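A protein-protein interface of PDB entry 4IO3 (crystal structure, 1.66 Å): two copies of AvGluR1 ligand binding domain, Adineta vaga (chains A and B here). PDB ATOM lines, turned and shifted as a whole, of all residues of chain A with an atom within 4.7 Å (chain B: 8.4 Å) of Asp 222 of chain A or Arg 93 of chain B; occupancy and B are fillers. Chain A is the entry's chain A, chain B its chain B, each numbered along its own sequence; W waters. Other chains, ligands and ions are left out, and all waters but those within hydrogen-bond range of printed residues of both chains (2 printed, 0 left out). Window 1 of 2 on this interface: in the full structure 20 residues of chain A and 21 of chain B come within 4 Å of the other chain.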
ATOM      1  N   SER A  99      24.987  13.306 -38.578  1.00  0.00           N
ATOM      2  CA  SER A  99      25.134  12.878 -37.202  1.00  0.00           C
ATOM      3  C   SER A  99      26.531  12.338 -36.941  1.00  0.00           C
ATOM      4  O   SER A  99      27.338  12.089 -37.850  1.00  0.00           O
ATOM      5  CB  SER A  99      24.122  11.782 -36.883  1.00  0.00           C
ATOM      6  OG  SER A  99      24.520  10.526 -37.448  1.00  0.00           O
ATOM      7  N   ASN A 100      26.840  12.129 -35.669  1.00  0.00           N
ATOM      8  CA  ASN A 100      27.994  11.339 -35.332  1.00  0.00           C
ATOM      9  C   ASN A 100      27.951  10.040 -36.094  1.00  0.00           C
ATOM     10  O   ASN A 100      26.893   9.480 -36.359  1.00  0.00           O
ATOM     11  CB  ASN A 100      27.990  11.024 -33.836  1.00  0.00           C
ATOM     12  CG  ASN A 100      28.401  12.197 -33.028  1.00  0.00           C
ATOM     13  OD1 ASN A 100      27.564  12.956 -32.542  1.00  0.00           O
ATOM     14  ND2 ASN A 100      29.700  12.380 -32.896  1.00  0.00           N
ATOM     15  N   ALA A 218      19.606  18.100 -33.547  1.00  0.00           N
ATOM     16  CA  ALA A 218      20.947  17.532 -33.755  1.00  0.00           C
ATOM     17  C   ALA A 218      21.515  16.885 -32.501  1.00  0.00           C
ATOM     18  O   ALA A 218      22.032  15.766 -32.555  1.00  0.00           O
ATOM     19  CB  ALA A 218      21.922  18.598 -34.288  1.00  0.00           C
ATOM     20  N   LYS A 219      21.436  17.594 -31.383  1.00  0.00           N
ATOM     21  CA  LYS A 219      21.980  17.059 -30.129  1.00  0.00           C
ATOM     22  C   LYS A 219      21.279  15.768 -29.687  1.00  0.00           C
ATOM     23  O   LYS A 219      21.941  14.799 -29.300  1.00  0.00           O
ATOM     24  CB  LYS A 219      21.913  18.100 -28.991  1.00  0.00           C
ATOM     25  CG  LYS A 219      22.514  17.581 -27.671  1.00  0.00           C
ATOM     26  CD  LYS A 219      22.050  18.379 -26.487  1.00  0.00           C
ATOM     27  CE  LYS A 219      20.613  18.065 -26.135  1.00  0.00           C
ATOM     28  NZ  LYS A 219      20.162  18.901 -25.000  1.00  0.00           N
ATOM     29  N   ASP A 220      19.948  15.737 -29.736  1.00  0.00           N
ATOM     30  CA  ASP A 220      19.184  14.565 -29.271  1.00  0.00           C
ATOM     31  C   ASP A 220      19.647  13.338 -30.064  1.00  0.00           C
ATOM     32  O   ASP A 220      19.926  12.272 -29.517  1.00  0.00           O
ATOM     33  CB  ASP A 220      17.660  14.801 -29.442  1.00  0.00           C
ATOM     34  CG  ASP A 220      16.769  13.773 -28.674  1.00  0.00           C
ATOM     35  OD1 ASP A 220      17.194  13.159 -27.677  1.00  0.00           O
ATOM     36  OD2 ASP A 220      15.581  13.593 -29.051  1.00  0.00           O
ATOM     37  N   LEU A 221      19.771  13.496 -31.375  1.00  0.00           N
ATOM     38  CA  LEU A 221      20.134  12.367 -32.215  1.00  0.00           C
ATOM     39  C   LEU A 221      21.561  11.916 -31.944  1.00  0.00           C
ATOM     40  O   LEU A 221      21.823  10.730 -31.812  1.00  0.00           O
ATOM     41  CB  LEU A 221      19.939  12.687 -33.699  1.00  0.00           C
ATOM     42  CG  LEU A 221      20.328  11.581 -34.681  1.00  0.00           C
ATOM     43  CD1 LEU A 221      19.524  10.293 -34.454  1.00  0.00           C
ATOM     44  CD2 LEU A 221      20.180  12.039 -36.136  1.00  0.00           C
ATOM     45  N   ASP A 222      22.494  12.873 -31.870  1.00  0.00           N
ATOM     46  CA  ASP A 222      23.893  12.527 -31.656  1.00  0.00           C
ATOM     47  C   ASP A 222      24.123  11.830 -30.306  1.00  0.00           C
ATOM     48  O   ASP A 222      24.862  10.840 -30.215  1.00  0.00           O
ATOM     49  CB  ASP A 222      24.791  13.767 -31.717  1.00  0.00           C
ATOM     50  CG  ASP A 222      25.099  14.211 -33.116  1.00  0.00           C
ATOM     51  OD1 ASP A 222      24.773  13.471 -34.066  1.00  0.00           O
ATOM     52  OD2 ASP A 222      25.692  15.325 -33.254  1.00  0.00           O
ATOM     53  N   VAL A 223      23.488  12.349 -29.254  1.00  0.00           N
ATOM     54  CA  VAL A 223      23.640  11.729 -27.948  1.00  0.00           C
ATOM     55  C   VAL A 223      23.176  10.285 -27.979  1.00  0.00           C
ATOM     56  O   VAL A 223      23.801   9.403 -27.388  1.00  0.00           O
ATOM     57  CB  VAL A 223      22.879  12.540 -26.890  1.00  0.00           C
ATOM     58  CG1 VAL A 223      22.690  11.768 -25.594  1.00  0.00           C
ATOM     59  CG2 VAL A 223      23.613  13.842 -26.631  1.00  0.00           C
ATOM     60  N   ASN A 224      22.080  10.039 -28.683  1.00  0.00           N
ATOM     61  CA  ASN A 224      21.550   8.704 -28.747  1.00  0.00           C
ATOM     62  C   ASN A 224      22.378   7.766 -29.593  1.00  0.00           C
ATOM     63  O   ASN A 224      22.570   6.591 -29.244  1.00  0.00           O
ATOM     64  CB  ASN A 224      20.084   8.737 -29.171  1.00  0.00           C
ATOM     65  CG  ASN A 224      19.172   9.050 -28.009  1.00  0.00           C
ATOM     66  OD1 ASN A 224      18.778   8.151 -27.286  1.00  0.00           O
ATOM     67  ND2 ASN A 224      18.870  10.319 -27.803  1.00  0.00           N
ATOM     68  N   ILE A 225      22.896   8.272 -30.717  1.00  0.00           N
ATOM     69  CA  ILE A 225      23.793   7.441 -31.518  1.00  0.00           C
ATOM     70  C   ILE A 225      25.040   7.052 -30.706  1.00  0.00           C
ATOM     71  O   ILE A 225      25.486   5.897 -30.689  1.00  0.00           O
ATOM     72  CB  ILE A 225      24.208   8.193 -32.791  1.00  0.00           C
ATOM     73  CG1 ILE A 225      23.016   8.295 -33.739  1.00  0.00           C
ATOM     74  CG2 ILE A 225      25.372   7.499 -33.455  1.00  0.00           C
ATOM     75  CD1 ILE A 225      22.579   6.928 -34.277  1.00  0.00           C
ATOM     76  N   LEU A 226      25.616   8.017 -29.998  1.00  0.00           N
ATOM     77  CA  LEU A 226      26.825   7.755 -29.224  1.00  0.00           C
ATOM     78  C   LEU A 226      26.535   6.772 -28.090  1.00  0.00           C
ATOM     79  O   LEU A 226      27.355   5.943 -27.742  1.00  0.00           O
ATOM     80  CB  LEU A 226      27.380   9.068 -28.682  1.00  0.00           C
ATOM     81  CG  LEU A 226      28.013   9.972 -29.745  1.00  0.00           C
ATOM     82  CD1 LEU A 226      28.238  11.383 -29.299  1.00  0.00           C
ATOM     83  CD2 LEU A 226      29.335   9.335 -30.191  1.00  0.00           C
ATOM     84  N   VAL B  71      36.635  20.097 -21.592  1.00  0.00           N
ATOM     85  CA  VAL B  71      35.339  20.172 -22.229  1.00  0.00           C
ATOM     86  C   VAL B  71      34.412  21.107 -21.432  1.00  0.00           C
ATOM     87  O   VAL B  71      33.704  21.953 -21.980  1.00  0.00           O
ATOM     88  CB  VAL B  71      34.732  18.769 -22.361  1.00  0.00           C
ATOM     89  CG1 VAL B  71      33.321  18.855 -22.859  1.00  0.00           C
ATOM     90  CG2 VAL B  71      35.552  17.923 -23.338  1.00  0.00           C
ATOM     91  N   THR B  87      38.061  12.369 -26.832  1.00  0.00           N
ATOM     92  CA  THR B  87      37.107  11.353 -27.245  1.00  0.00           C
ATOM     93  C   THR B  87      35.680  11.892 -27.295  1.00  0.00           C
ATOM     94  O   THR B  87      35.216  12.569 -26.386  1.00  0.00           O
ATOM     95  CB  THR B  87      37.182  10.125 -26.308  1.00  0.00           C
ATOM     96  OG1 THR B  87      38.520   9.637 -26.296  1.00  0.00           O
ATOM     97  CG2 THR B  87      36.273   9.030 -26.767  1.00  0.00           C
ATOM     98  N   VAL B  88      34.992  11.595 -28.386  1.00  0.00           N
ATOM     99  CA  VAL B  88      33.599  11.960 -28.537  1.00  0.00           C
ATOM    100  C   VAL B  88      32.745  11.007 -27.718  1.00  0.00           C
ATOM    101  O   VAL B  88      32.708   9.782 -27.965  1.00  0.00           O
ATOM    102  CB  VAL B  88      33.180  11.929 -30.015  1.00  0.00           C
ATOM    103  CG1 VAL B  88      31.769  12.364 -30.133  1.00  0.00           C
ATOM    104  CG2 VAL B  88      34.080  12.803 -30.845  1.00  0.00           C
ATOM    105  N   THR B  89      32.067  11.530 -26.708  1.00  0.00           N
ATOM    106  CA  THR B  89      31.229  10.675 -25.884  1.00  0.00           C
ATOM    107  C   THR B  89      29.845  11.246 -25.779  1.00  0.00           C
ATOM    108  O   THR B  89      29.621  12.455 -25.978  1.00  0.00           O
ATOM    109  CB  THR B  89      31.797  10.497 -24.427  1.00  0.00           C
ATOM    110  OG1 THR B  89      31.588  11.744 -23.745  1.00  0.00           O
ATOM    111  CG2 THR B  89      33.287  10.120 -24.428  1.00  0.00           C
ATOM    112  N   SER B  90      28.895  10.384 -25.492  1.00  0.00           N
ATOM    113  CA  SER B  90      27.526  10.792 -25.321  1.00  0.00           C
ATOM    114  C   SER B  90      27.362  11.886 -24.253  1.00  0.00           C
ATOM    115  O   SER B  90      26.720  12.904 -24.477  1.00  0.00           O
ATOM    116  CB  SER B  90      26.713   9.561 -24.966  1.00  0.00           C
ATOM    117  OG  SER B  90      25.339   9.840 -25.039  1.00  0.00           O
ATOM    118  N   ALA B  91      27.984  11.673 -23.105  1.00  0.00           N
ATOM    119  CA  ALA B  91      27.873  12.600 -22.002  1.00  0.00           C
ATOM    120  C   ALA B  91      28.417  13.982 -22.384  1.00  0.00           C
ATOM    121  O   ALA B  91      27.866  15.011 -22.015  1.00  0.00           O
ATOM    122  CB  ALA B  91      28.620  12.037 -20.775  1.00  0.00           C
ATOM    123  N   ARG B  92      29.527  14.007 -23.116  1.00  0.00           N
ATOM    124  CA  ARG B  92      30.093  15.279 -23.523  1.00  0.00           C
ATOM    125  C   ARG B  92      29.221  15.940 -24.578  1.00  0.00           C
ATOM    126  O   ARG B  92      29.072  17.157 -24.594  1.00  0.00           O
ATOM    127  CB  ARG B  92      31.496  15.061 -24.063  1.00  0.00           C
ATOM    128  CG  ARG B  92      32.485  14.713 -22.958  1.00  0.00           C
ATOM    129  CD  ARG B  92      33.828  14.205 -23.489  1.00  0.00           C
ATOM    130  NE  ARG B  92      34.724  13.883 -22.373  1.00  0.00           N
ATOM    131  CZ  ARG B  92      35.956  13.429 -22.548  1.00  0.00           C
ATOM    132  NH1 ARG B  92      36.389  13.214 -23.778  1.00  0.00           N
ATOM    133  NH2 ARG B  92      36.757  13.183 -21.510  1.00  0.00           N
ATOM    134  N   ARG B  93      28.629  15.136 -25.456  1.00  0.00           N
ATOM    135  CA  ARG B  93      27.822  15.685 -26.555  1.00  0.00           C
ATOM    136  C   ARG B  93      26.553  16.392 -26.027  1.00  0.00           C
ATOM    137  O   ARG B  93      25.989  17.269 -26.684  1.00  0.00           O
ATOM    138  CB  ARG B  93      27.489  14.569 -27.561  1.00  0.00           C
ATOM    139  CG  ARG B  93      26.620  15.028 -28.745  1.00  0.00           C
ATOM    140  CD  ARG B  93      27.384  15.946 -29.681  1.00  0.00           C
ATOM    141  NE  ARG B  93      26.530  16.501 -30.722  1.00  0.00           N
ATOM    142  CZ  ARG B  93      25.823  17.613 -30.605  1.00  0.00           C
ATOM    143  NH1 ARG B  93      25.810  18.331 -29.487  1.00  0.00           N
ATOM    144  NH2 ARG B  93      25.104  18.028 -31.640  1.00  0.00           N
ATOM    145  N   GLU B  94      26.143  16.048 -24.798  1.00  0.00           N
ATOM    146  CA  GLU B  94      25.024  16.719 -24.149  1.00  0.00           C
ATOM    147  C   GLU B  94      25.340  18.209 -23.957  1.00  0.00           C
ATOM    148  O   GLU B  94      24.423  19.058 -23.981  1.00  0.00           O
ATOM    149  CB  GLU B  94      24.737  16.024 -22.818  1.00  0.00           C
ATOM    150  CG  GLU B  94      23.429  16.327 -22.215  1.00  0.00           C
ATOM    151  CD  GLU B  94      22.930  15.155 -21.380  1.00  0.00           C
ATOM    152  OE1 GLU B  94      23.773  14.390 -20.856  1.00  0.00           O
ATOM    153  OE2 GLU B  94      21.700  14.972 -21.269  1.00  0.00           O
ATOM    154  N   ILE B  95      26.618  18.540 -23.781  1.00  0.00           N
ATOM    155  CA  ILE B  95      26.977  19.915 -23.408  1.00  0.00           C
ATOM    156  C   ILE B  95      27.835  20.709 -24.408  1.00  0.00           C
ATOM    157  O   ILE B  95      27.944  21.934 -24.279  1.00  0.00           O
ATOM    158  CB  ILE B  95      27.649  19.943 -21.988  1.00  0.00           C
ATOM    159  CG1 ILE B  95      29.001  19.235 -22.036  1.00  0.00           C
ATOM    160  CG2 ILE B  95      26.692  19.307 -20.946  1.00  0.00           C
ATOM    161  CD1 ILE B  95      29.892  19.543 -20.801  1.00  0.00           C
ATOM    162  N   VAL B  96      28.443  20.018 -25.382  1.00  0.00           N
ATOM    163  CA  VAL B  96      29.238  20.635 -26.456  1.00  0.00           C
ATOM    164  C   VAL B  96      28.947  19.878 -27.743  1.00  0.00           C
ATOM    165  O   VAL B  96      28.425  18.769 -27.701  1.00  0.00           O
ATOM    166  CB  VAL B  96      30.780  20.581 -26.216  1.00  0.00           C
ATOM    167  CG1 VAL B  96      31.214  21.398 -24.954  1.00  0.00           C
ATOM    168  CG2 VAL B  96      31.254  19.144 -26.103  1.00  0.00           C
ATOM    169  N   ALA B  97      29.272  20.494 -28.871  1.00  0.00           N
ATOM    170  CA  ALA B  97      29.260  19.809 -30.145  1.00  0.00           C
ATOM    171  C   ALA B  97      30.667  19.351 -30.517  1.00  0.00           C
ATOM    172  O   ALA B  97      31.669  19.761 -29.920  1.00  0.00           O
ATOM    173  CB  ALA B  97      28.667  20.696 -31.236  1.00  0.00           C
ATOM    174  N   PHE B  98      30.735  18.446 -31.498  1.00  0.00           N
ATOM    175  CA  PHE B  98      32.029  17.994 -31.987  1.00  0.00           C
ATOM    176  C   PHE B  98      32.072  18.100 -33.507  1.00  0.00           C
ATOM    177  O   PHE B  98      31.061  17.861 -34.183  1.00  0.00           O
ATOM    178  CB  PHE B  98      32.292  16.530 -31.618  1.00  0.00           C
ATOM    179  CG  PHE B  98      32.540  16.281 -30.168  1.00  0.00           C
ATOM    180  CD1 PHE B  98      31.483  16.008 -29.302  1.00  0.00           C
ATOM    181  CD2 PHE B  98      33.843  16.275 -29.656  1.00  0.00           C
ATOM    182  CE1 PHE B  98      31.718  15.774 -27.980  1.00  0.00           C
ATOM    183  CE2 PHE B  98      34.075  16.000 -28.322  1.00  0.00           C
ATOM    184  CZ  PHE B  98      33.006  15.735 -27.485  1.00  0.00           C
ATOM    185  N   SER B  99      33.230  18.436 -34.051  1.00  0.00           N
ATOM    186  CA  SER B  99      33.432  18.389 -35.494  1.00  0.00           C
ATOM    187  C   SER B  99      33.402  16.965 -35.991  1.00  0.00           C
ATOM    188  O   SER B  99      33.418  16.003 -35.221  1.00  0.00           O
ATOM    189  CB  SER B  99      34.807  18.959 -35.812  1.00  0.00           C
ATOM    190  OG  SER B  99      35.832  18.014 -35.520  1.00  0.00           O
ATOM    191  N   VAL B 210      36.243  19.944 -30.273  1.00  0.00           N
ATOM    192  CA  VAL B 210      35.138  20.388 -29.442  1.00  0.00           C
ATOM    193  C   VAL B 210      34.765  21.801 -29.847  1.00  0.00           C
ATOM    194  O   VAL B 210      35.645  22.660 -30.010  1.00  0.00           O
ATOM    195  CB  VAL B 210      35.528  20.382 -27.929  1.00  0.00           C
ATOM    196  CG1 VAL B 210      34.339  20.784 -27.061  1.00  0.00           C
ATOM    197  CG2 VAL B 210      36.022  19.024 -27.535  1.00  0.00           C
ATOM    198  N   THR B 211      33.470  22.034 -30.015  1.00  0.00           N
ATOM    199  CA  THR B 211      32.945  23.361 -30.313  1.00  0.00           C
ATOM    200  C   THR B 211      31.720  23.640 -29.450  1.00  0.00           C
ATOM    201  O   THR B 211      31.160  22.744 -28.839  1.00  0.00           O
ATOM    202  CB  THR B 211      32.529  23.513 -31.795  1.00  0.00           C
ATOM    203  OG1 THR B 211      31.247  22.930 -32.014  1.00  0.00           O
ATOM    204  CG2 THR B 211      33.495  22.831 -32.725  1.00  0.00           C
ATOM    205  N   PRO B 212      31.291  24.897 -29.400  1.00  0.00           N
ATOM    206  CA  PRO B 212      30.033  25.180 -28.714  1.00  0.00           C
ATOM    207  C   PRO B 212      28.876  24.502 -29.417  1.00  0.00           C
ATOM    208  O   PRO B 212      28.959  24.240 -30.625  1.00  0.00           O
ATOM    209  CB  PRO B 212      29.899  26.704 -28.832  1.00  0.00           C
ATOM    210  CG  PRO B 212      31.321  27.184 -29.028  1.00  0.00           C
ATOM    211  CD  PRO B 212      31.981  26.127 -29.841  1.00  0.00           C
ATOM    212  N   LYS B 213      27.828  24.170 -28.677  1.00  0.00           N
ATOM    213  CA  LYS B 213      26.611  23.683 -29.321  1.00  0.00           C
ATOM    214  C   LYS B 213      26.029  24.759 -30.242  1.00  0.00           C
ATOM    215  O   LYS B 213      26.175  25.943 -29.983  1.00  0.00           O
ATOM    216  CB  LYS B 213      25.575  23.242 -28.283  1.00  0.00           C
ATOM    217  CG  LYS B 213      26.033  22.028 -27.514  1.00  0.00           C
ATOM    218  CD  LYS B 213      24.921  21.366 -26.740  1.00  0.00           C
ATOM    219  CE  LYS B 213      24.391  22.277 -25.655  1.00  0.00           C
ATOM    220  NZ  LYS B 213      23.326  21.538 -24.925  1.00  0.00           N
ATOM    221  N   GLU B 214      25.398  24.327 -31.331  1.00  0.00           N
ATOM    222  CA  GLU B 214      24.766  25.249 -32.291  1.00  0.00           C
ATOM    223  C   GLU B 214      25.706  26.367 -32.735  1.00  0.00           C
ATOM    224  O   GLU B 214      25.326  27.543 -32.804  1.00  0.00           O
ATOM    225  CB  GLU B 214      23.472  25.820 -31.705  1.00  0.00           C
ATOM    226  CG  GLU B 214      22.440  24.734 -31.373  1.00  0.00           C
ATOM    227  CD  GLU B 214      21.396  25.193 -30.364  1.00  0.00           C
ATOM    228  OE1 GLU B 214      20.957  26.361 -30.424  1.00  0.00           O
ATOM    229  OE2 GLU B 214      21.026  24.386 -29.490  1.00  0.00           O
ATOM    230  N   TRP B 215      26.932  25.990 -33.059  1.00  0.00           N
ATOM    231  CA  TRP B 215      27.987  26.963 -33.354  1.00  0.00           C
ATOM    232  C   TRP B 215      27.821  27.569 -34.742  1.00  0.00           C
ATOM    233  O   TRP B 215      27.581  26.853 -35.716  1.00  0.00           O
ATOM    234  CB  TRP B 215      29.333  26.265 -33.324  1.00  0.00           C
ATOM    235  CG  TRP B 215      30.544  27.134 -33.243  1.00  0.00           C
ATOM    236  CD1 TRP B 215      30.693  28.290 -32.541  1.00  0.00           C
ATOM    237  CD2 TRP B 215      31.802  26.874 -33.859  1.00  0.00           C
ATOM    238  NE1 TRP B 215      31.978  28.758 -32.672  1.00  0.00           N
ATOM    239  CE2 TRP B 215      32.676  27.906 -33.483  1.00  0.00           C
ATOM    240  CE3 TRP B 215      32.280  25.853 -34.690  1.00  0.00           C
ATOM    241  CZ2 TRP B 215      33.989  27.960 -33.920  1.00  0.00           C
ATOM    242  CZ3 TRP B 215      33.587  25.909 -35.119  1.00  0.00           C
ATOM    243  CH2 TRP B 215      34.428  26.952 -34.744  1.00  0.00           C
HETATM  244  O   HOH W   1      21.069  21.628 -26.524  1.00  0.00           O
HETATM  245  O   HOH W   2      31.803  14.015 -34.681  1.00  0.00           O
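OG of Ser 90 of chain B sits at hydrogen-bond distance from O of Val 223 of chain A (2.8 Å). NE of Arg 93 of chain B lies within salt-bridge range of OD2 of Asp 222 of chain A.
The guanidinium group of Arg 93 of chain B sits at hydrogen-bond distance from the backbone carbonyl oxygen of Val 96 of chain B (3.2 Å). The side-chain amino group (NZ) of Lys 213 of chain B sits at hydrogen-bond distance from the backbone carbonyl oxygen (O) of Glu 94 of chain B (2.9 Å). The backbone NH (N) of Asn 100 of chain A sits at hydrogen-bond distance from the side-chain carboxylate (OD1) of Asp 222 of chain A. The side-chain hydroxyl (OG1) of Thr 89 of chain B lies within hydrogen-bond range of the backbone NH (N) of Arg 92 of chain B, 3.1 Å away.
Among the printed residues, merely in contact across the chains: Asn 100 of chain A with Val 88 of chain B, Lys 219 of chain A with Glu 94 of chain B, Lys 219 of chain A with Arg 93 of chain B, Leu 226 of chain A with Arg 93 of chain B, Lys 219 of chain A with Lys 213 of chain B, Leu 226 of chain A with Thr 89 of chain B, Leu 226 of chain A with Val 88 of chain B, Leu 226 of chain A with Ser 90 of chain B, Val 223 of chain A with Glu 94 of chain B, Val 223 of chain A with Arg 93 of chain B and Ala 218 of chain A with Arg 93 of chain B.
Of the printed residues of chain B, Asn 100 of chain A touches Val 88. Of the printed residues of chain B, Ala 218 of chain A touches Arg 93. Leu 221 of chain A touches none of the printed residues of chain B. Ile 225 of chain A touches none of the printed residues of chain B. Of the printed residues of chain B, Leu 226 of chain A touches Val 88, Thr 89, Ser 90 and Arg 93. Printed residues of chain A within 4 Å of Thr 89 of chain B: Leu 226 (3.8 Å). The nearest printed residue of chain B that does not touch Asp 222 of chain A is Ser 90 of chain B (5.3 Å). The nearest printed residue of chain B that does not touch Asn 100 of chain A is Arg 93 of chain B (4.1 Å).
Of the 11 printed residues of chain A, 6 touch a printed residue of chain B. Hydrophobic or aromatic side chains of chain A that line the printed part of chain B: Val 223 and Leu 226. Along chain A the printed residues that touch a printed residue of chain B span positions 100 to 226. Printed residues of chain B that touch a printed residue of chain A: Val 88, Thr 89, Ser 90, Arg 93, Glu 94 and Lys 213. Hydrophobic or aromatic side chains of chain B that line the printed part of chain A: Val 88. Among the printed residues, 13 pairs touch across the chains. Among the printed residues, Asp or Glu carboxylates within 4 Å of a Lys or Arg side-chain nitrogen of the other chain: Asp 222 of chain A with Arg 93 of chain B.
Position printed for both chains: 99. Of the 13 pairs that touch across the chains among the printed residues, none has its exchanged pair printed and touching as well.
Water W2 lies within hydrogen-bond range of the backbone carbonyl oxygen (O) of Ser 99 of chain B and the side-chain amide nitrogen (ND2) of Asn 100 of chain A. Water W1 bridges the side-chain amino group of Lys 213 of chain B (2.8 Å) and the side-chain amino group of Lys 219 of chain A (3.3 Å).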
